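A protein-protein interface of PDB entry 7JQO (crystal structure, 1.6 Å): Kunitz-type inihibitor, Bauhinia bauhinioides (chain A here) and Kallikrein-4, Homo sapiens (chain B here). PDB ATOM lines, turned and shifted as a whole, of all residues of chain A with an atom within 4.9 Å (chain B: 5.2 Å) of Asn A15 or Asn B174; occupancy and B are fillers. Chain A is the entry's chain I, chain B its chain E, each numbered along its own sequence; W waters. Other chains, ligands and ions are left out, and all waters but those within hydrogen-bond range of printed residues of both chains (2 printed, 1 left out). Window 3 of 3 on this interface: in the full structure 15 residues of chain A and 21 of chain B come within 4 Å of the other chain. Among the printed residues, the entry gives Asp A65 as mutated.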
ATOM      1  N   VAL A  13     -11.079  19.465  -6.048  1.00  0.00           N
ATOM      2  CA  VAL A  13      -9.712  19.013  -6.286  1.00  0.00           C
ATOM      3  C   VAL A  13      -9.547  17.621  -5.667  1.00  0.00           C
ATOM      4  O   VAL A  13      -9.944  17.397  -4.520  1.00  0.00           O
ATOM      5  CB  VAL A  13      -8.719  20.040  -5.698  1.00  0.00           C
ATOM      6  CG1 VAL A  13      -7.271  19.520  -5.605  1.00  0.00           C
ATOM      7  CG2 VAL A  13      -8.793  21.345  -6.495  1.00  0.00           C
ATOM      8  N   SER A  14      -8.967  16.689  -6.435  1.00  0.00           N
ATOM      9  CA  SER A  14      -8.819  15.322  -5.950  1.00  0.00           C
ATOM     10  C   SER A  14      -7.665  15.186  -4.948  1.00  0.00           C
ATOM     11  O   SER A  14      -6.712  15.975  -4.934  1.00  0.00           O
ATOM     12  CB  SER A  14      -8.766  14.288  -7.048  1.00  0.00           C
ATOM     13  OG  SER A  14      -7.567  14.399  -7.729  1.00  0.00           O
ATOM     14  N   ASN A  15      -7.770  14.130  -4.126  1.00  0.00           N
ATOM     15  CA  ASN A  15      -6.740  13.774  -3.165  1.00  0.00           C
ATOM     16  C   ASN A  15      -5.727  12.878  -3.894  1.00  0.00           C
ATOM     17  O   ASN A  15      -5.901  11.650  -3.966  1.00  0.00           O
ATOM     18  CB  ASN A  15      -7.375  13.104  -1.939  1.00  0.00           C
ATOM     19  CG  ASN A  15      -6.357  12.723  -0.887  1.00  0.00           C
ATOM     20  OD1 ASN A  15      -5.164  13.014  -1.033  1.00  0.00           O
ATOM     21  ND2 ASN A  15      -6.825  12.054   0.164  1.00  0.00           N
ATOM     22  N   GLY A  16      -4.689  13.505  -4.457  1.00  0.00           N
ATOM     23  CA  GLY A  16      -3.536  12.812  -5.024  1.00  0.00           C
ATOM     24  C   GLY A  16      -3.712  12.290  -6.451  1.00  0.00           C
ATOM     25  O   GLY A  16      -2.734  12.199  -7.198  1.00  0.00           O
ATOM     26  N   ALA A  17      -4.949  11.989  -6.853  1.00  0.00           N
ATOM     27  CA  ALA A  17      -5.194  11.214  -8.068  1.00  0.00           C
ATOM     28  C   ALA A  17      -4.933  12.031  -9.333  1.00  0.00           C
ATOM     29  O   ALA A  17      -4.489  11.488 -10.343  1.00  0.00           O
ATOM     30  CB  ALA A  17      -6.620  10.706  -8.061  1.00  0.00           C
ATOM     31  N   PHE A  60      -2.019  17.304  -4.575  1.00  0.00           N
ATOM     32  CA  PHE A  60      -2.315  17.619  -3.182  1.00  0.00           C
ATOM     33  C   PHE A  60      -2.711  16.317  -2.493  1.00  0.00           C
ATOM     34  O   PHE A  60      -3.597  15.611  -2.976  1.00  0.00           O
ATOM     35  CB  PHE A  60      -3.505  18.578  -3.099  1.00  0.00           C
ATOM     36  CG  PHE A  60      -3.298  19.867  -3.868  1.00  0.00           C
ATOM     37  CD1 PHE A  60      -2.626  20.948  -3.300  1.00  0.00           C
ATOM     38  CD2 PHE A  60      -3.788  19.986  -5.169  1.00  0.00           C
ATOM     39  CE1 PHE A  60      -2.465  22.138  -4.023  1.00  0.00           C
ATOM     40  CE2 PHE A  60      -3.629  21.167  -5.889  1.00  0.00           C
ATOM     41  CZ  PHE A  60      -2.983  22.252  -5.309  1.00  0.00           C
ATOM     42  N   GLU A  61      -2.040  15.977  -1.379  1.00  0.00           N
ATOM     43  CA  GLU A  61      -2.215  14.651  -0.790  1.00  0.00           C
ATOM     44  C   GLU A  61      -2.533  14.779   0.708  1.00  0.00           C
ATOM     45  O   GLU A  61      -1.835  15.465   1.463  1.00  0.00           O
ATOM     46  CB  GLU A  61      -0.932  13.804  -0.952  1.00  0.00           C
ATOM     47  CG  GLU A  61      -0.568  13.514  -2.425  1.00  0.00           C
ATOM     48  CD  GLU A  61       0.577  12.525  -2.647  1.00  0.00           C
ATOM     49  OE1 GLU A  61       1.375  12.330  -1.703  1.00  0.00           O
ATOM     50  OE2 GLU A  61       0.628  11.895  -3.746  1.00  0.00           O
ATOM     51  N   SER A  62      -3.557  14.042   1.134  1.00  0.00           N
ATOM     52  CA  SER A  62      -3.920  13.835   2.531  1.00  0.00           C
ATOM     53  C   SER A  62      -3.984  12.319   2.773  1.00  0.00           C
ATOM     54  O   SER A  62      -4.436  11.563   1.899  1.00  0.00           O
ATOM     55  CB  SER A  62      -5.288  14.461   2.794  1.00  0.00           C
ATOM     56  OG  SER A  62      -5.831  13.980   4.020  1.00  0.00           O
ATOM     57  N   LEU A  64      -6.081  10.875   4.621  1.00  0.00           N
ATOM     58  CA  LEU A  64      -7.490  10.534   4.796  1.00  0.00           C
ATOM     59  C   LEU A  64      -7.998   9.766   3.569  1.00  0.00           C
ATOM     60  O   LEU A  64      -7.625  10.088   2.432  1.00  0.00           O
ATOM     61  CB  LEU A  64      -8.311  11.823   4.963  1.00  0.00           C
ATOM     62  CG  LEU A  64      -7.932  12.694   6.189  1.00  0.00           C
ATOM     63  CD1 LEU A  64      -8.637  14.054   6.113  1.00  0.00           C
ATOM     64  CD2 LEU A  64      -8.278  11.972   7.514  1.00  0.00           C
ATOM     65  N   ASP A  65      -8.881   8.788   3.810  1.00  0.00           N
ATOM     66  CA  ASP A  65      -9.381   7.932   2.725  1.00  0.00           C
ATOM     67  C   ASP A  65     -10.543   8.567   1.949  1.00  0.00           C
ATOM     68  O   ASP A  65     -11.511   7.883   1.566  1.00  0.00           O
ATOM     69  CB  ASP A  65      -9.708   6.544   3.272  1.00  0.00           C
ATOM     70  CG  ASP A  65      -8.448   5.714   3.406  1.00  0.00           C
ATOM     71  OD1 ASP A  65      -7.603   5.686   2.425  1.00  0.00           O
ATOM     72  OD2 ASP A  65      -8.272   5.150   4.502  1.00  0.00           O
ATOM     73  N   ILE A  66     -10.426   9.868   1.694  1.00  0.00           N
ATOM     74  CA  ILE A  66     -11.423  10.642   0.963  1.00  0.00           C
ATOM     75  C   ILE A  66     -10.798  11.065  -0.364  1.00  0.00           C
ATOM     76  O   ILE A  66      -9.567  11.131  -0.475  1.00  0.00           O
ATOM     77  CB  ILE A  66     -11.878  11.837   1.836  1.00  0.00           C
ATOM     78  CG1 ILE A  66     -13.114  12.552   1.255  1.00  0.00           C
ATOM     79  CG2 ILE A  66     -10.718  12.811   2.115  1.00  0.00           C
ATOM     80  CD1 ILE A  66     -13.719  13.550   2.215  1.00  0.00           C
ATOM     81  N   ASN A  67     -11.596  11.271  -1.428  1.00  0.00           N
ATOM     82  CA  ASN A  67     -10.973  11.635  -2.696  1.00  0.00           C
ATOM     83  C   ASN A  67     -11.213  13.105  -3.062  1.00  0.00           C
ATOM     84  O   ASN A  67     -11.152  13.456  -4.245  1.00  0.00           O
ATOM     85  CB  ASN A  67     -11.319  10.698  -3.864  1.00  0.00           C
ATOM     86  CG  ASN A  67     -10.232  10.650  -4.930  1.00  0.00           C
ATOM     87  OD1 ASN A  67      -9.073  11.014  -4.669  1.00  0.00           O
ATOM     88  ND2 ASN A  67     -10.591  10.190  -6.130  1.00  0.00           N
ATOM     89  N   ILE A  68     -11.495  13.956  -2.065  1.00  0.00           N
ATOM     90  CA  ILE A  68     -11.520  15.406  -2.272  1.00  0.00           C
ATOM     91  C   ILE A  68     -10.680  16.056  -1.176  1.00  0.00           C
ATOM     92  O   ILE A  68     -10.327  15.398  -0.189  1.00  0.00           O
ATOM     93  CB  ILE A  68     -12.965  15.961  -2.262  1.00  0.00           C
ATOM     94  CG1 ILE A  68     -13.607  15.753  -0.887  1.00  0.00           C
ATOM     95  CG2 ILE A  68     -13.779  15.366  -3.416  1.00  0.00           C
ATOM     96  CD1 ILE A  68     -14.948  16.428  -0.720  1.00  0.00           C
ATOM     97  N   ILE A  69     -10.359  17.342  -1.348  1.00  0.00           N
ATOM     98  CA  ILE A  69      -9.548  18.099  -0.394  1.00  0.00           C
ATOM     99  C   ILE A  69     -10.398  19.239   0.175  1.00  0.00           C
ATOM    100  O   ILE A  69     -11.061  19.956  -0.595  1.00  0.00           O
ATOM    101  CB  ILE A  69      -8.301  18.654  -1.136  1.00  0.00           C
ATOM    102  CG1 ILE A  69      -7.430  17.498  -1.648  1.00  0.00           C
ATOM    103  CG2 ILE A  69      -7.545  19.662  -0.292  1.00  0.00           C
ATOM    104  CD1 ILE A  69      -6.936  16.594  -0.573  1.00  0.00           C
ATOM    105  N   GLY B 124     -15.157   3.312  -2.942  1.00  0.00           N
ATOM    106  CA  GLY B 124     -13.907   3.999  -3.253  1.00  0.00           C
ATOM    107  C   GLY B 124     -13.049   3.276  -4.305  1.00  0.00           C
ATOM    108  O   GLY B 124     -13.459   2.281  -4.920  1.00  0.00           O
ATOM    109  N   LEU B 125     -11.826   3.782  -4.520  1.00  0.00           N
ATOM    110  CA  LEU B 125     -11.000   3.383  -5.655  1.00  0.00           C
ATOM    111  C   LEU B 125     -10.641   1.905  -5.593  1.00  0.00           C
ATOM    112  O   LEU B 125     -10.390   1.354  -4.505  1.00  0.00           O
ATOM    113  CB  LEU B 125      -9.700   4.198  -5.685  1.00  0.00           C
ATOM    114  CG  LEU B 125      -9.891   5.694  -5.918  1.00  0.00           C
ATOM    115  CD1 LEU B 125      -8.547   6.408  -5.908  1.00  0.00           C
ATOM    116  CD2 LEU B 125     -10.601   5.954  -7.265  1.00  0.00           C
ATOM    117  N   MET B 131     -13.185   3.951 -10.187  1.00  0.00           N
ATOM    118  CA  MET B 131     -14.265   3.770  -9.237  1.00  0.00           C
ATOM    119  C   MET B 131     -15.139   2.601  -9.691  1.00  0.00           C
ATOM    120  O   MET B 131     -15.403   2.437 -10.893  1.00  0.00           O
ATOM    121  CB  MET B 131     -15.120   5.036  -9.116  1.00  0.00           C
ATOM    122  CG  MET B 131     -14.316   6.210  -8.584  1.00  0.00           C
ATOM    123  SD  MET B 131     -14.029   6.033  -6.790  1.00  0.00           S
ATOM    124  CE  MET B 131     -15.499   6.878  -6.175  1.00  0.00           C
ATOM    125  N   SER B 172      -8.818  -0.714   2.277  1.00  0.00           N
ATOM    126  CA  SER B 172      -9.721   0.362   1.886  1.00  0.00           C
ATOM    127  C   SER B 172      -8.932   1.441   1.139  1.00  0.00           C
ATOM    128  O   SER B 172      -7.702   1.464   1.218  1.00  0.00           O
ATOM    129  CB  SER B 172     -10.420   0.894   3.126  1.00  0.00           C
ATOM    130  OG  SER B 172      -9.449   1.321   4.057  1.00  0.00           O
ATOM    131  N   CSO B 173      -9.607   2.323   0.374  1.00  0.00           N
ATOM    132  CA  CSO B 173      -8.885   3.332  -0.398  1.00  0.00           C
ATOM    133  CB  CSO B 173      -8.515   2.813  -1.795  1.00  0.00           C
ATOM    134  SG  CSO B 173      -7.131   3.636  -2.655  1.00  0.00           S
ATOM    135  C   CSO B 173      -9.697   4.631  -0.475  1.00  0.00           C
ATOM    136  O   CSO B 173     -10.747   4.767   0.153  1.00  0.00           O
ATOM    137  OD  CSO B 173      -6.949   5.259  -2.450  1.00  0.00           O
ATOM    138  N   ASN B 174      -9.223   5.590  -1.275  1.00  0.00           N
ATOM    139  CA  ASN B 174      -9.876   6.894  -1.298  1.00  0.00           C
ATOM    140  C   ASN B 174     -11.299   6.776  -1.832  1.00  0.00           C
ATOM    141  O   ASN B 174     -11.551   6.169  -2.888  1.00  0.00           O
ATOM    142  CB  ASN B 174      -9.045   7.937  -2.050  1.00  0.00           C
ATOM    143  CG  ASN B 174      -7.628   8.028  -1.509  1.00  0.00           C
ATOM    144  OD1 ASN B 174      -7.312   8.906  -0.695  1.00  0.00           O
ATOM    145  ND2 ASN B 174      -6.781   7.089  -1.909  1.00  0.00           N
ATOM    146  N   GLY B 175     -12.223   7.400  -1.093  1.00  0.00           N
ATOM    147  CA  GLY B 175     -13.660   7.314  -1.338  1.00  0.00           C
ATOM    148  C   GLY B 175     -14.325   6.272  -0.446  1.00  0.00           C
ATOM    149  O   GLY B 175     -15.544   6.255  -0.366  1.00  0.00           O
ATOM    150  N   ASP B 176     -13.527   5.485   0.309  1.00  0.00           N
ATOM    151  CA  ASP B 176     -14.105   4.551   1.278  1.00  0.00           C
ATOM    152  C   ASP B 176     -14.274   5.189   2.667  1.00  0.00           C
ATOM    153  O   ASP B 176     -14.927   4.561   3.532  1.00  0.00           O
ATOM    154  CB  ASP B 176     -13.215   3.287   1.393  1.00  0.00           C
ATOM    155  CG  ASP B 176     -13.281   2.445   0.119  1.00  0.00           C
ATOM    156  OD1 ASP B 176     -14.421   2.328  -0.468  1.00  0.00           O
ATOM    157  OD2 ASP B 176     -12.251   1.846  -0.264  1.00  0.00           O
HETATM  158  O   HOH W   1      -8.516   2.916   6.401  1.00  0.00           O
HETATM  159  O   HOH W   2      -6.754   2.748   4.090  1.00  0.00           O
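Of the 8 printed residues of chain B, 4 touch a printed residue of chain A. Among the printed residues, 9 pairs touch across the chains.
OD1 of Asn B174 sits close to O of Ile A66. N of Asp B176 lies within hydrogen-bond range of O of Asp A65 (3.4 Å). The backbone carbonyl oxygen of Leu A64 lies close to the side-chain amide oxygen of Asn B174, at 3.4 Å. The backbone NH (N) of Gly B175 is in hydrogen-bond range of the backbone carbonyl oxygen (O) of Asp A65, 2.8 Å away. The side-chain amide oxygen of Asn B174 sits at hydrogen-bond distance from the side-chain amide nitrogen of Asn A15, 3.3 Å away.
Among the printed residues, merely in contact across the chains: Asp A65 with Asn B174, Asp A65 with CSO B173, Ile A66 with Gly B175 and Asn A67 with Gly B175.
OD1 of Asn A15 lies within hydrogen-bond range of N of Ser A62 (2.9 Å). O of Asn B174 sits at hydrogen-bond distance from N of Leu B125 (2.9 Å). The backbone NH of Gly B124 sits at hydrogen-bond distance from the side-chain carboxylate of Asp B176. N of CSO B173 sits at hydrogen-bond distance from the side-chain carboxylate of Asp B176 (2.8 Å). ND2 of Asn A15 sits at hydrogen-bond distance from O of Ile A66 (3.0 Å). ND2 of Asn A15 is in hydrogen-bond range of O of Leu A64 (3.1 Å).
Of the printed residues of chain B, Asn A15 touches Asn B174 (3.3 Å). Of the printed residues of chain A, Asn B174 touches Asn A15 (3.3 Å), Leu A64 (3.4 Å), Asp A65 (3.4 Å) and Ile A66 (3.2 Å). Of the printed residues of chain A, Gly B175 touches Asp A65 (2.8 Å), Ile A66 (3.9 Å) and Asn A67 (3.9 Å). Printed residues of chain B within 4 Å of Ile A66: Asn B174 and Gly B175. Of the printed residues of chain B, Asp A65 touches CSO B173, Asn B174, Gly B175 and Asp B176. Printed residues of chain B within 4 Å of Leu A64: Asn B174 (3.4 Å). Leu B125 touches none of the printed residues of chain A. The nearest printed residue of chain B that does not touch Asn A15 is Leu B125 (6.2 Å).
Water W2 lies within hydrogen-bond range of OD2 of Asp A65 (2.9 Å) and OG of Ser B172 (3.0 Å). Water W1 lies within hydrogen-bond range of OD2 of Asp A65 (2.9 Å) and OG of Ser B172 (3.0 Å).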
